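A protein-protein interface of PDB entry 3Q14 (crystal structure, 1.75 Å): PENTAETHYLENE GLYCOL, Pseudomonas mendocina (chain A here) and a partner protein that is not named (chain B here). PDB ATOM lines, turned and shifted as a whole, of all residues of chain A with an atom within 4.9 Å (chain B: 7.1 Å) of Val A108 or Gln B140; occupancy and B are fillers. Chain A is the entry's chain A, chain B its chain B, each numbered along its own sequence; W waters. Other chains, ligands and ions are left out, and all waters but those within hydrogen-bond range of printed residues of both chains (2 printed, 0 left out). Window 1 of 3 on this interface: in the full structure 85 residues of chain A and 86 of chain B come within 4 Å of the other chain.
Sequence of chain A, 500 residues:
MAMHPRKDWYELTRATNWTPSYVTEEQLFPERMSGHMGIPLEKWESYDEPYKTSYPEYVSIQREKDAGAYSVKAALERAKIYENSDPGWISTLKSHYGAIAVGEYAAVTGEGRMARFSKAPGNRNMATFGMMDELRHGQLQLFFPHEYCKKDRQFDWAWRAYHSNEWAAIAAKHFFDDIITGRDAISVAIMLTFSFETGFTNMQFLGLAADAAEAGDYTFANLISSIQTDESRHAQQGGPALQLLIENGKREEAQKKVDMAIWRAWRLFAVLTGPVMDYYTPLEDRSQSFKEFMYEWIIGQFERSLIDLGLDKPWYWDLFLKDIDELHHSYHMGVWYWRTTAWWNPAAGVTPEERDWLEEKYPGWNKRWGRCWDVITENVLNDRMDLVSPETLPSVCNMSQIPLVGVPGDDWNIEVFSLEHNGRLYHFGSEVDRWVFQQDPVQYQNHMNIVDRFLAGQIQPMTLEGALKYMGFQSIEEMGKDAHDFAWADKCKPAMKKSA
Of the 22 printed residues of chain B, 7 touch a printed residue of chain A.
Hydrophobic or aromatic side chains of chain B within 4 Å of the printed part of chain A: His B33, Tyr B55 and Ile B153.
Of the 12 printed residues of chain A, 6 touch a printed residue of chain B.
Printed residues of chain A that touch a printed residue of chain B: Tyr A105, Val A108, Thr A109, Gly A112, Met A131 and Leu A135.
Hydrophobic or aromatic side chains of chain A within 4 Å of the printed part of chain B: Tyr A105, Val A108, Met A131 and Leu A135.
Among the printed residues, no Asp or Glu carboxylate lies within 4 Å of a Lys or Arg side-chain nitrogen of the other chain.
His B33 touches Tyr A105.
Ser B149 touches Tyr A105.
CG1 of Val A108 touches NE2 of Gln B140, 3.6 Å away.
CD1 of Ile B153 touches CG1 of Val A108, 3.6 Å away.
Thr A109 touches Tyr B55 (CG2 to OH, 3.9 Å).
Gly A112 touches Gln B140.
Met A131 touches Gln B140 (CE to OE1, 3.6 Å).
Asn B150 touches Leu A135.
Ile B153 touches Leu A135.
A ring nitrogen (NE2) of His B33 sits close to the backbone carbonyl oxygen of Ala B143, at 3.4 Å.
The side-chain hydroxyl of Ser B149 is in hydrogen-bond range of a ring nitrogen (NE2) of His B33 (2.8 Å).
O of Gln B141 sits at hydrogen-bond distance from OH of Tyr B55, at 2.9 Å.
O of Ala B137 lies close to OE1 of Gln B140 (3.4 Å).
The backbone carbonyl oxygen of Ala B137 sits close to the side-chain amide oxygen of Gln B141, at 2.9 Å.
The side-chain hydroxyl of Ser B149 is in hydrogen-bond range of the backbone carbonyl oxygen of Gln B140 (2.8 Å).
ND2 of Asn B150 sits at hydrogen-bond distance from OH of Tyr A105 (2.6 Å).
The side-chain hydroxyl (OG1) of Thr A109 lies within hydrogen-bond range of the side-chain amide nitrogen (NE2) of Gln B140.
O of Gly A112 lies close to OE1 of Gln B141 (2.9 Å).
Water W1 lies within hydrogen-bond range of the backbone carbonyl oxygen of Gln B141, the side-chain hydroxyl of Thr A109 and the side-chain hydroxyl of Tyr B55.
Water W2 bridges NE2 of Gln B140 and OH of Tyr A105.
Val A108 touches just these residues of chain B: Gln B140 (3.6 Å) and Ile B153 (3.6 Å).
Of the printed residues of chain B, Gly A112 touches Gln B140 (3.5 Å) and Gln B141 (2.9 Å).
Ser B136 touches none of the printed residues of chain A.
Printed residues of chain A within 4 Å of Gln B140: Val A108 (3.6 Å), Thr A109 (3.3 Å), Gly A112 (3.5 Å) and Met A131 (3.6 Å).
Of the printed residues of chain A, Ser B149 touches Tyr A105 (3.6 Å).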
ATOM      1  N   GLU A 104     -31.531  20.944 -26.124  1.00  0.00           N
ATOM      2  CA  GLU A 104     -30.199  21.217 -26.661  1.00  0.00           C
ATOM      3  C   GLU A 104     -29.244  21.470 -25.510  1.00  0.00           C
ATOM      4  O   GLU A 104     -28.123  20.975 -25.490  1.00  0.00           O
ATOM      5  CB  GLU A 104     -30.205  22.451 -27.568  1.00  0.00           C
ATOM      6  CG  GLU A 104     -31.082  22.307 -28.788  1.00  0.00           C
ATOM      7  CD  GLU A 104     -30.324  21.810 -29.993  1.00  0.00           C
ATOM      8  OE1 GLU A 104     -30.797  22.055 -31.115  1.00  0.00           O
ATOM      9  OE2 GLU A 104     -29.260  21.176 -29.818  1.00  0.00           O
ATOM     10  N   TYR A 105     -29.679  22.268 -24.543  1.00  0.00           N
ATOM     11  CA  TYR A 105     -28.790  22.576 -23.443  1.00  0.00           C
ATOM     12  C   TYR A 105     -28.491  21.304 -22.646  1.00  0.00           C
ATOM     13  O   TYR A 105     -27.362  21.091 -22.190  1.00  0.00           O
ATOM     14  CB  TYR A 105     -29.359  23.684 -22.539  1.00  0.00           C
ATOM     15  CG  TYR A 105     -28.340  24.107 -21.520  1.00  0.00           C
ATOM     16  CD1 TYR A 105     -27.261  24.921 -21.878  1.00  0.00           C
ATOM     17  CD2 TYR A 105     -28.424  23.655 -20.204  1.00  0.00           C
ATOM     18  CE1 TYR A 105     -26.308  25.287 -20.935  1.00  0.00           C
ATOM     19  CE2 TYR A 105     -27.483  24.011 -19.273  1.00  0.00           C
ATOM     20  CZ  TYR A 105     -26.429  24.814 -19.638  1.00  0.00           C
ATOM     21  OH  TYR A 105     -25.500  25.137 -18.679  1.00  0.00           O
ATOM     22  N   ALA A 106     -29.494  20.440 -22.498  1.00  0.00           N
ATOM     23  CA  ALA A 106     -29.262  19.136 -21.878  1.00  0.00           C
ATOM     24  C   ALA A 106     -28.226  18.306 -22.636  1.00  0.00           C
ATOM     25  O   ALA A 106     -27.453  17.577 -22.029  1.00  0.00           O
ATOM     26  CB  ALA A 106     -30.573  18.343 -21.737  1.00  0.00           C
ATOM     27  N   ALA A 107     -28.203  18.415 -23.959  1.00  0.00           N
ATOM     28  CA  ALA A 107     -27.224  17.663 -24.741  1.00  0.00           C
ATOM     29  C   ALA A 107     -25.791  18.071 -24.417  1.00  0.00           C
ATOM     30  O   ALA A 107     -24.855  17.319 -24.695  1.00  0.00           O
ATOM     31  CB  ALA A 107     -27.496  17.816 -26.241  1.00  0.00           C
ATOM     32  N   VAL A 108     -25.607  19.261 -23.838  1.00  0.00           N
ATOM     33  CA  VAL A 108     -24.267  19.642 -23.406  1.00  0.00           C
ATOM     34  C   VAL A 108     -23.759  18.596 -22.430  1.00  0.00           C
ATOM     35  O   VAL A 108     -22.581  18.220 -22.443  1.00  0.00           O
ATOM     36  CB  VAL A 108     -24.224  21.014 -22.697  1.00  0.00           C
ATOM     37  CG1 VAL A 108     -22.819  21.263 -22.156  1.00  0.00           C
ATOM     38  CG2 VAL A 108     -24.626  22.125 -23.650  1.00  0.00           C
ATOM     39  N   THR A 109     -24.665  18.135 -21.573  1.00  0.00           N
ATOM     40  CA  THR A 109     -24.326  17.119 -20.566  1.00  0.00           C
ATOM     41  C   THR A 109     -23.945  15.766 -21.179  1.00  0.00           C
ATOM     42  O   THR A 109     -23.014  15.109 -20.715  1.00  0.00           O
ATOM     43  CB  THR A 109     -25.447  16.983 -19.527  1.00  0.00           C
ATOM     44  OG1 THR A 109     -25.447  18.149 -18.691  1.00  0.00           O
ATOM     45  CG2 THR A 109     -25.238  15.739 -18.626  1.00  0.00           C
ATOM     46  N   GLY A 110     -24.653  15.347 -22.218  1.00  0.00           N
ATOM     47  CA  GLY A 110     -24.276  14.132 -22.925  1.00  0.00           C
ATOM     48  C   GLY A 110     -22.866  14.264 -23.501  1.00  0.00           C
ATOM     49  O   GLY A 110     -22.036  13.342 -23.410  1.00  0.00           O
ATOM     50  N   GLU A 111     -22.587  15.406 -24.114  1.00  0.00           N
ATOM     51  CA  GLU A 111     -21.252  15.639 -24.665  1.00  0.00           C
ATOM     52  C   GLU A 111     -20.223  15.689 -23.538  1.00  0.00           C
ATOM     53  O   GLU A 111     -19.138  15.125 -23.658  1.00  0.00           O
ATOM     54  CB  GLU A 111     -21.220  16.913 -25.506  1.00  0.00           C
ATOM     55  CG  GLU A 111     -22.047  16.820 -26.795  1.00  0.00           C
ATOM     56  CD  GLU A 111     -21.384  15.973 -27.891  1.00  0.00           C
ATOM     57  OE1 GLU A 111     -20.194  15.634 -27.756  1.00  0.00           O
ATOM     58  OE2 GLU A 111     -22.059  15.648 -28.891  1.00  0.00           O
ATOM     59  N   GLY A 112     -20.578  16.336 -22.428  1.00  0.00           N
ATOM     60  CA  GLY A 112     -19.689  16.400 -21.283  1.00  0.00           C
ATOM     61  C   GLY A 112     -19.368  15.031 -20.712  1.00  0.00           C
ATOM     62  O   GLY A 112     -18.251  14.781 -20.268  1.00  0.00           O
ATOM     63  N   MET A 131     -19.786  19.860 -26.748  1.00  0.00           N
ATOM     64  CA  MET A 131     -20.331  20.633 -25.626  1.00  0.00           C
ATOM     65  C   MET A 131     -20.582  22.071 -26.070  1.00  0.00           C
ATOM     66  O   MET A 131     -21.617  22.664 -25.770  1.00  0.00           O
ATOM     67  CB  MET A 131     -19.350  20.646 -24.451  1.00  0.00           C
ATOM     68  CG  MET A 131     -19.157  19.285 -23.770  1.00  0.00           C
ATOM     69  SD  MET A 131     -17.742  19.317 -22.647  1.00  0.00           S
ATOM     70  CE  MET A 131     -18.357  20.393 -21.349  1.00  0.00           C
ATOM     71  N   GLU A 134     -23.610  22.391 -28.534  1.00  0.00           N
ATOM     72  CA  GLU A 134     -24.938  22.301 -27.935  1.00  0.00           C
ATOM     73  C   GLU A 134     -25.226  23.542 -27.093  1.00  0.00           C
ATOM     74  O   GLU A 134     -26.369  23.971 -26.982  1.00  0.00           O
ATOM     75  CB  GLU A 134     -25.114  21.020 -27.105  1.00  0.00           C
ATOM     76  CG  GLU A 134     -24.887  19.697 -27.879  1.00  0.00           C
ATOM     77  CD  GLU A 134     -25.820  19.490 -29.078  1.00  0.00           C
ATOM     78  OE1 GLU A 134     -26.607  20.393 -29.448  1.00  0.00           O
ATOM     79  OE2 GLU A 134     -25.784  18.379 -29.636  1.00  0.00           O
ATOM     80  N   LEU A 135     -24.184  24.125 -26.515  1.00  0.00           N
ATOM     81  CA  LEU A 135     -24.331  25.412 -25.834  1.00  0.00           C
ATOM     82  C   LEU A 135     -24.833  26.451 -26.841  1.00  0.00           C
ATOM     83  O   LEU A 135     -25.794  27.173 -26.583  1.00  0.00           O
ATOM     84  CB  LEU A 135     -22.997  25.858 -25.220  1.00  0.00           C
ATOM     85  CG  LEU A 135     -23.050  27.199 -24.470  1.00  0.00           C
ATOM     86  CD1 LEU A 135     -23.977  27.098 -23.272  1.00  0.00           C
ATOM     87  CD2 LEU A 135     -21.661  27.617 -24.032  1.00  0.00           C
ATOM     88  N   HIS B  33     -31.011  24.167 -15.898  1.00  0.00           N
ATOM     89  CA  HIS B  33     -30.917  22.790 -15.391  1.00  0.00           C
ATOM     90  C   HIS B  33     -32.237  22.338 -14.768  1.00  0.00           C
ATOM     91  O   HIS B  33     -32.466  22.570 -13.581  1.00  0.00           O
ATOM     92  CB  HIS B  33     -29.855  22.659 -14.301  1.00  0.00           C
ATOM     93  CG  HIS B  33     -28.444  22.638 -14.794  1.00  0.00           C
ATOM     94  ND1 HIS B  33     -28.104  22.351 -16.100  1.00  0.00           N
ATOM     95  CD2 HIS B  33     -27.280  22.862 -14.141  1.00  0.00           C
ATOM     96  CE1 HIS B  33     -26.789  22.405 -16.229  1.00  0.00           C
ATOM     97  NE2 HIS B  33     -26.267  22.718 -15.056  1.00  0.00           N
ATOM     98  N   TYR B  55     -26.477  11.427  -9.392  1.00  0.00           N
ATOM     99  CA  TYR B  55     -26.739  12.840  -9.147  1.00  0.00           C
ATOM    100  C   TYR B  55     -27.217  13.094  -7.729  1.00  0.00           C
ATOM    101  O   TYR B  55     -26.820  14.083  -7.101  1.00  0.00           O
ATOM    102  CB  TYR B  55     -27.710  13.428 -10.174  1.00  0.00           C
ATOM    103  CG  TYR B  55     -26.979  13.838 -11.426  1.00  0.00           C
ATOM    104  CD1 TYR B  55     -26.389  12.881 -12.241  1.00  0.00           C
ATOM    105  CD2 TYR B  55     -26.846  15.186 -11.777  1.00  0.00           C
ATOM    106  CE1 TYR B  55     -25.693  13.250 -13.388  1.00  0.00           C
ATOM    107  CE2 TYR B  55     -26.152  15.561 -12.924  1.00  0.00           C
ATOM    108  CZ  TYR B  55     -25.585  14.586 -13.720  1.00  0.00           C
ATOM    109  OH  TYR B  55     -24.897  14.922 -14.855  1.00  0.00           O
ATOM    110  N   ARG B  59     -24.289  15.394  -6.586  1.00  0.00           N
ATOM    111  CA  ARG B  59     -24.710  16.784  -6.676  1.00  0.00           C
ATOM    112  C   ARG B  59     -25.567  17.156  -5.471  1.00  0.00           C
ATOM    113  O   ARG B  59     -25.158  17.981  -4.653  1.00  0.00           O
ATOM    114  CB  ARG B  59     -25.459  17.085  -7.975  1.00  0.00           C
ATOM    115  CG  ARG B  59     -25.962  18.531  -8.020  1.00  0.00           C
ATOM    116  CD  ARG B  59     -27.051  18.722  -9.050  1.00  0.00           C
ATOM    117  NE  ARG B  59     -26.505  19.022 -10.369  1.00  0.00           N
ATOM    118  CZ  ARG B  59     -27.188  18.895 -11.504  1.00  0.00           C
ATOM    119  NH1 ARG B  59     -28.443  18.452 -11.471  1.00  0.00           N
ATOM    120  NH2 ARG B  59     -26.611  19.202 -12.666  1.00  0.00           N
ATOM    121  N   MET B 134     -10.689  17.363 -19.089  1.00  0.00           N
ATOM    122  CA  MET B 134     -11.583  16.316 -18.587  1.00  0.00           C
ATOM    123  C   MET B 134     -12.255  16.751 -17.297  1.00  0.00           C
ATOM    124  O   MET B 134     -13.449  16.508 -17.081  1.00  0.00           O
ATOM    125  CB  MET B 134     -10.810  15.017 -18.325  1.00  0.00           C
ATOM    126  CG  MET B 134     -10.342  14.335 -19.605  1.00  0.00           C
ATOM    127  SD  MET B 134      -9.161  13.009 -19.289  1.00  0.00           S
ATOM    128  CE  MET B 134     -10.136  11.822 -18.351  1.00  0.00           C
ATOM    129  N   SER B 135     -11.465  17.364 -16.426  1.00  0.00           N
ATOM    130  CA  SER B 135     -11.947  17.709 -15.101  1.00  0.00           C
ATOM    131  C   SER B 135     -12.973  18.829 -15.191  1.00  0.00           C
ATOM    132  O   SER B 135     -13.997  18.809 -14.499  1.00  0.00           O
ATOM    133  CB  SER B 135     -10.787  18.100 -14.186  1.00  0.00           C
ATOM    134  OG  SER B 135     -11.257  18.281 -12.862  1.00  0.00           O
ATOM    135  N   SER B 136     -12.707  19.794 -16.070  1.00  0.00           N
ATOM    136  CA  SER B 136     -13.640  20.886 -16.294  1.00  0.00           C
ATOM    137  C   SER B 136     -14.965  20.369 -16.831  1.00  0.00           C
ATOM    138  O   SER B 136     -16.029  20.865 -16.460  1.00  0.00           O
ATOM    139  CB  SER B 136     -13.036  21.920 -17.255  1.00  0.00           C
ATOM    140  OG  SER B 136     -11.911  22.529 -16.635  1.00  0.00           O
ATOM    141  N   ALA B 137     -14.897  19.365 -17.700  1.00  0.00           N
ATOM    142  CA  ALA B 137     -16.113  18.786 -18.256  1.00  0.00           C
ATOM    143  C   ALA B 137     -16.907  18.097 -17.156  1.00  0.00           C
ATOM    144  O   ALA B 137     -18.133  18.093 -17.182  1.00  0.00           O
ATOM    145  CB  ALA B 137     -15.778  17.795 -19.365  1.00  0.00           C
ATOM    146  N   TYR B 138     -16.214  17.511 -16.186  1.00  0.00           N
ATOM    147  CA  TYR B 138     -16.935  16.872 -15.089  1.00  0.00           C
ATOM    148  C   TYR B 138     -17.653  17.908 -14.216  1.00  0.00           C
ATOM    149  O   TYR B 138     -18.817  17.730 -13.835  1.00  0.00           O
ATOM    150  CB  TYR B 138     -16.028  15.987 -14.233  1.00  0.00           C
ATOM    151  CG  TYR B 138     -16.839  15.270 -13.179  1.00  0.00           C
ATOM    152  CD1 TYR B 138     -16.803  15.665 -11.843  1.00  0.00           C
ATOM    153  CD2 TYR B 138     -17.698  14.242 -13.539  1.00  0.00           C
ATOM    154  CE1 TYR B 138     -17.579  15.013 -10.892  1.00  0.00           C
ATOM    155  CE2 TYR B 138     -18.468  13.589 -12.610  1.00  0.00           C
ATOM    156  CZ  TYR B 138     -18.414  13.979 -11.293  1.00  0.00           C
ATOM    157  OH  TYR B 138     -19.196  13.314 -10.383  1.00  0.00           O
ATOM    158  N   VAL B 139     -16.973  18.997 -13.890  1.00  0.00           N
ATOM    159  CA  VAL B 139     -17.653  20.018 -13.110  1.00  0.00           C
ATOM    160  C   VAL B 139     -18.863  20.544 -13.897  1.00  0.00           C
ATOM    161  O   VAL B 139     -19.929  20.749 -13.314  1.00  0.00           O
ATOM    162  CB  VAL B 139     -16.722  21.152 -12.667  1.00  0.00           C
ATOM    163  CG1 VAL B 139     -17.475  22.099 -11.711  1.00  0.00           C
ATOM    164  CG2 VAL B 139     -15.501  20.577 -11.971  1.00  0.00           C
ATOM    165  N   GLN B 140     -18.715  20.718 -15.213  1.00  0.00           N
ATOM    166  CA  GLN B 140     -19.837  21.148 -16.045  1.00  0.00           C
ATOM    167  C   GLN B 140     -21.058  20.275 -15.812  1.00  0.00           C
ATOM    168  O   GLN B 140     -22.163  20.768 -15.582  1.00  0.00           O
ATOM    169  CB  GLN B 140     -19.487  21.095 -17.549  1.00  0.00           C
ATOM    170  CG  GLN B 140     -20.695  21.302 -18.486  1.00  0.00           C
ATOM    171  CD  GLN B 140     -21.432  20.000 -18.825  1.00  0.00           C
ATOM    172  OE1 GLN B 140     -20.815  18.968 -19.107  1.00  0.00           O
ATOM    173  NE2 GLN B 140     -22.762  20.046 -18.776  1.00  0.00           N
ATOM    174  N   GLN B 141     -20.872  18.967 -15.906  1.00  0.00           N
ATOM    175  CA  GLN B 141     -22.035  18.092 -15.928  1.00  0.00           C
ATOM    176  C   GLN B 141     -22.688  17.943 -14.557  1.00  0.00           C
ATOM    177  O   GLN B 141     -23.856  17.604 -14.461  1.00  0.00           O
ATOM    178  CB  GLN B 141     -21.696  16.734 -16.560  1.00  0.00           C
ATOM    179  CG  GLN B 141     -20.662  15.933 -15.808  1.00  0.00           C
ATOM    180  CD  GLN B 141     -19.934  14.965 -16.742  1.00  0.00           C
ATOM    181  OE1 GLN B 141     -19.064  15.370 -17.519  1.00  0.00           O
ATOM    182  NE2 GLN B 141     -20.290  13.698 -16.675  1.00  0.00           N
ATOM    183  N   MET B 142     -21.939  18.237 -13.505  1.00  0.00           N
ATOM    184  CA  MET B 142     -22.424  18.018 -12.147  1.00  0.00           C
ATOM    185  C   MET B 142     -22.897  19.297 -11.456  1.00  0.00           C
ATOM    186  O   MET B 142     -23.626  19.231 -10.464  1.00  0.00           O
ATOM    187  CB  MET B 142     -21.337  17.356 -11.285  1.00  0.00           C
ATOM    188  CG  MET B 142     -20.898  15.982 -11.779  1.00  0.00           C
ATOM    189  SD  MET B 142     -22.268  14.839 -12.096  1.00  0.00           S
ATOM    190  CE  MET B 142     -23.134  14.906 -10.536  1.00  0.00           C
ATOM    191  N   ALA B 143     -22.487  20.458 -11.955  1.00  0.00           N
ATOM    192  CA  ALA B 143     -22.766  21.710 -11.234  1.00  0.00           C
ATOM    193  C   ALA B 143     -24.264  21.961 -11.142  1.00  0.00           C
ATOM    194  O   ALA B 143     -25.007  21.623 -12.052  1.00  0.00           O
ATOM    195  CB  ALA B 143     -22.062  22.888 -11.911  1.00  0.00           C
ATOM    196  N   PRO B 144     -24.724  22.542 -10.025  1.00  0.00           N
ATOM    197  CA  PRO B 144     -26.167  22.668  -9.807  1.00  0.00           C
ATOM    198  C   PRO B 144     -26.845  23.917 -10.385  1.00  0.00           C
ATOM    199  O   PRO B 144     -27.990  24.186 -10.016  1.00  0.00           O
ATOM    200  CB  PRO B 144     -26.276  22.687  -8.271  1.00  0.00           C
ATOM    201  CG  PRO B 144     -25.001  23.345  -7.836  1.00  0.00           C
ATOM    202  CD  PRO B 144     -23.947  22.822  -8.804  1.00  0.00           C
ATOM    203  N   ALA B 145     -26.176  24.670 -11.261  1.00  0.00           N
ATOM    204  CA  ALA B 145     -26.829  25.787 -11.945  1.00  0.00           C
ATOM    205  C   ALA B 145     -26.255  25.925 -13.345  1.00  0.00           C
ATOM    206  O   ALA B 145     -25.067  25.701 -13.545  1.00  0.00           O
ATOM    207  CB  ALA B 145     -26.605  27.095 -11.191  1.00  0.00           C
ATOM    208  N   ILE B 148     -23.318  28.248 -13.652  1.00  0.00           N
ATOM    209  CA  ILE B 148     -22.056  27.661 -13.227  1.00  0.00           C
ATOM    210  C   ILE B 148     -21.514  26.739 -14.330  1.00  0.00           C
ATOM    211  O   ILE B 148     -20.346  26.826 -14.723  1.00  0.00           O
ATOM    212  CB  ILE B 148     -22.206  26.856 -11.925  1.00  0.00           C
ATOM    213  CG1 ILE B 148     -22.737  27.757 -10.798  1.00  0.00           C
ATOM    214  CG2 ILE B 148     -20.867  26.250 -11.540  1.00  0.00           C
ATOM    215  CD1 ILE B 148     -23.208  26.959  -9.556  1.00  0.00           C
ATOM    216  N   SER B 149     -22.366  25.851 -14.826  1.00  0.00           N
ATOM    217  CA  SER B 149     -21.955  24.916 -15.875  1.00  0.00           C
ATOM    218  C   SER B 149     -21.413  25.631 -17.105  1.00  0.00           C
ATOM    219  O   SER B 149     -20.455  25.151 -17.714  1.00  0.00           O
ATOM    220  CB  SER B 149     -23.109  23.995 -16.276  1.00  0.00           C
ATOM    221  OG  SER B 149     -23.495  23.193 -15.169  1.00  0.00           O
ATOM    222  N   ASN B 150     -22.008  26.768 -17.466  1.00  0.00           N
ATOM    223  CA  ASN B 150     -21.548  27.513 -18.654  1.00  0.00           C
ATOM    224  C   ASN B 150     -20.101  27.969 -18.493  1.00  0.00           C
ATOM    225  O   ASN B 150     -19.310  27.873 -19.433  1.00  0.00           O
ATOM    226  CB  ASN B 150     -22.448  28.715 -18.958  1.00  0.00           C
ATOM    227  CG  ASN B 150     -23.787  28.319 -19.587  1.00  0.00           C
ATOM    228  OD1 ASN B 150     -24.581  29.187 -19.985  1.00  0.00           O
ATOM    229  ND2 ASN B 150     -24.032  27.027 -19.705  1.00  0.00           N
ATOM    230  N   CYS B 151     -19.747  28.453 -17.301  1.00  0.00           N
ATOM    231  CA  CYS B 151     -18.357  28.836 -17.048  1.00  0.00           C
ATOM    232  C   CYS B 151     -17.441  27.635 -17.225  1.00  0.00           C
ATOM    233  O   CYS B 151     -16.342  27.766 -17.754  1.00  0.00           O
ATOM    234  CB  CYS B 151     -18.177  29.414 -15.636  1.00  0.00           C
ATOM    235  SG  CYS B 151     -19.052  30.969 -15.403  1.00  0.00           S
ATOM    236  N   CYS B 152     -17.899  26.467 -16.775  1.00  0.00           N
ATOM    237  CA  CYS B 152     -17.134  25.229 -16.917  1.00  0.00           C
ATOM    238  C   CYS B 152     -16.989  24.783 -18.369  1.00  0.00           C
ATOM    239  O   CYS B 152     -15.952  24.240 -18.743  1.00  0.00           O
ATOM    240  CB  CYS B 152     -17.786  24.097 -16.131  1.00  0.00           C
ATOM    241  SG  CYS B 152     -17.784  24.373 -14.367  1.00  0.00           S
ATOM    242  N   ILE B 153     -18.030  24.977 -19.173  1.00  0.00           N
ATOM    243  CA  ILE B 153     -17.950  24.623 -20.594  1.00  0.00           C
ATOM    244  C   ILE B 153     -16.850  25.438 -21.270  1.00  0.00           C
ATOM    245  O   ILE B 153     -16.020  24.896 -22.001  1.00  0.00           O
ATOM    246  CB  ILE B 153     -19.269  24.877 -21.346  1.00  0.00           C
ATOM    247  CG1 ILE B 153     -20.408  24.026 -20.773  1.00  0.00           C
ATOM    248  CG2 ILE B 153     -19.083  24.612 -22.875  1.00  0.00           C
ATOM    249  CD1 ILE B 153     -21.772  24.529 -21.200  1.00  0.00           C
ATOM    250  N   THR B 156     -13.531  24.272 -20.192  1.00  0.00           N
ATOM    251  CA  THR B 156     -13.168  23.020 -20.856  1.00  0.00           C
ATOM    252  C   THR B 156     -12.596  23.357 -22.238  1.00  0.00           C
ATOM    253  O   THR B 156     -11.574  22.802 -22.659  1.00  0.00           O
ATOM    254  CB  THR B 156     -14.396  22.094 -21.022  1.00  0.00           C
ATOM    255  OG1 THR B 156     -14.979  21.841 -19.735  1.00  0.00           O
ATOM    256  CG2 THR B 156     -14.001  20.752 -21.670  1.00  0.00           C
HETATM  257  O   HOH W   1     -25.891  17.677 -16.095  1.00  0.00           O
HETATM  258  O   HOH W   2     -24.606  22.316 -18.719  1.00  0.00           O
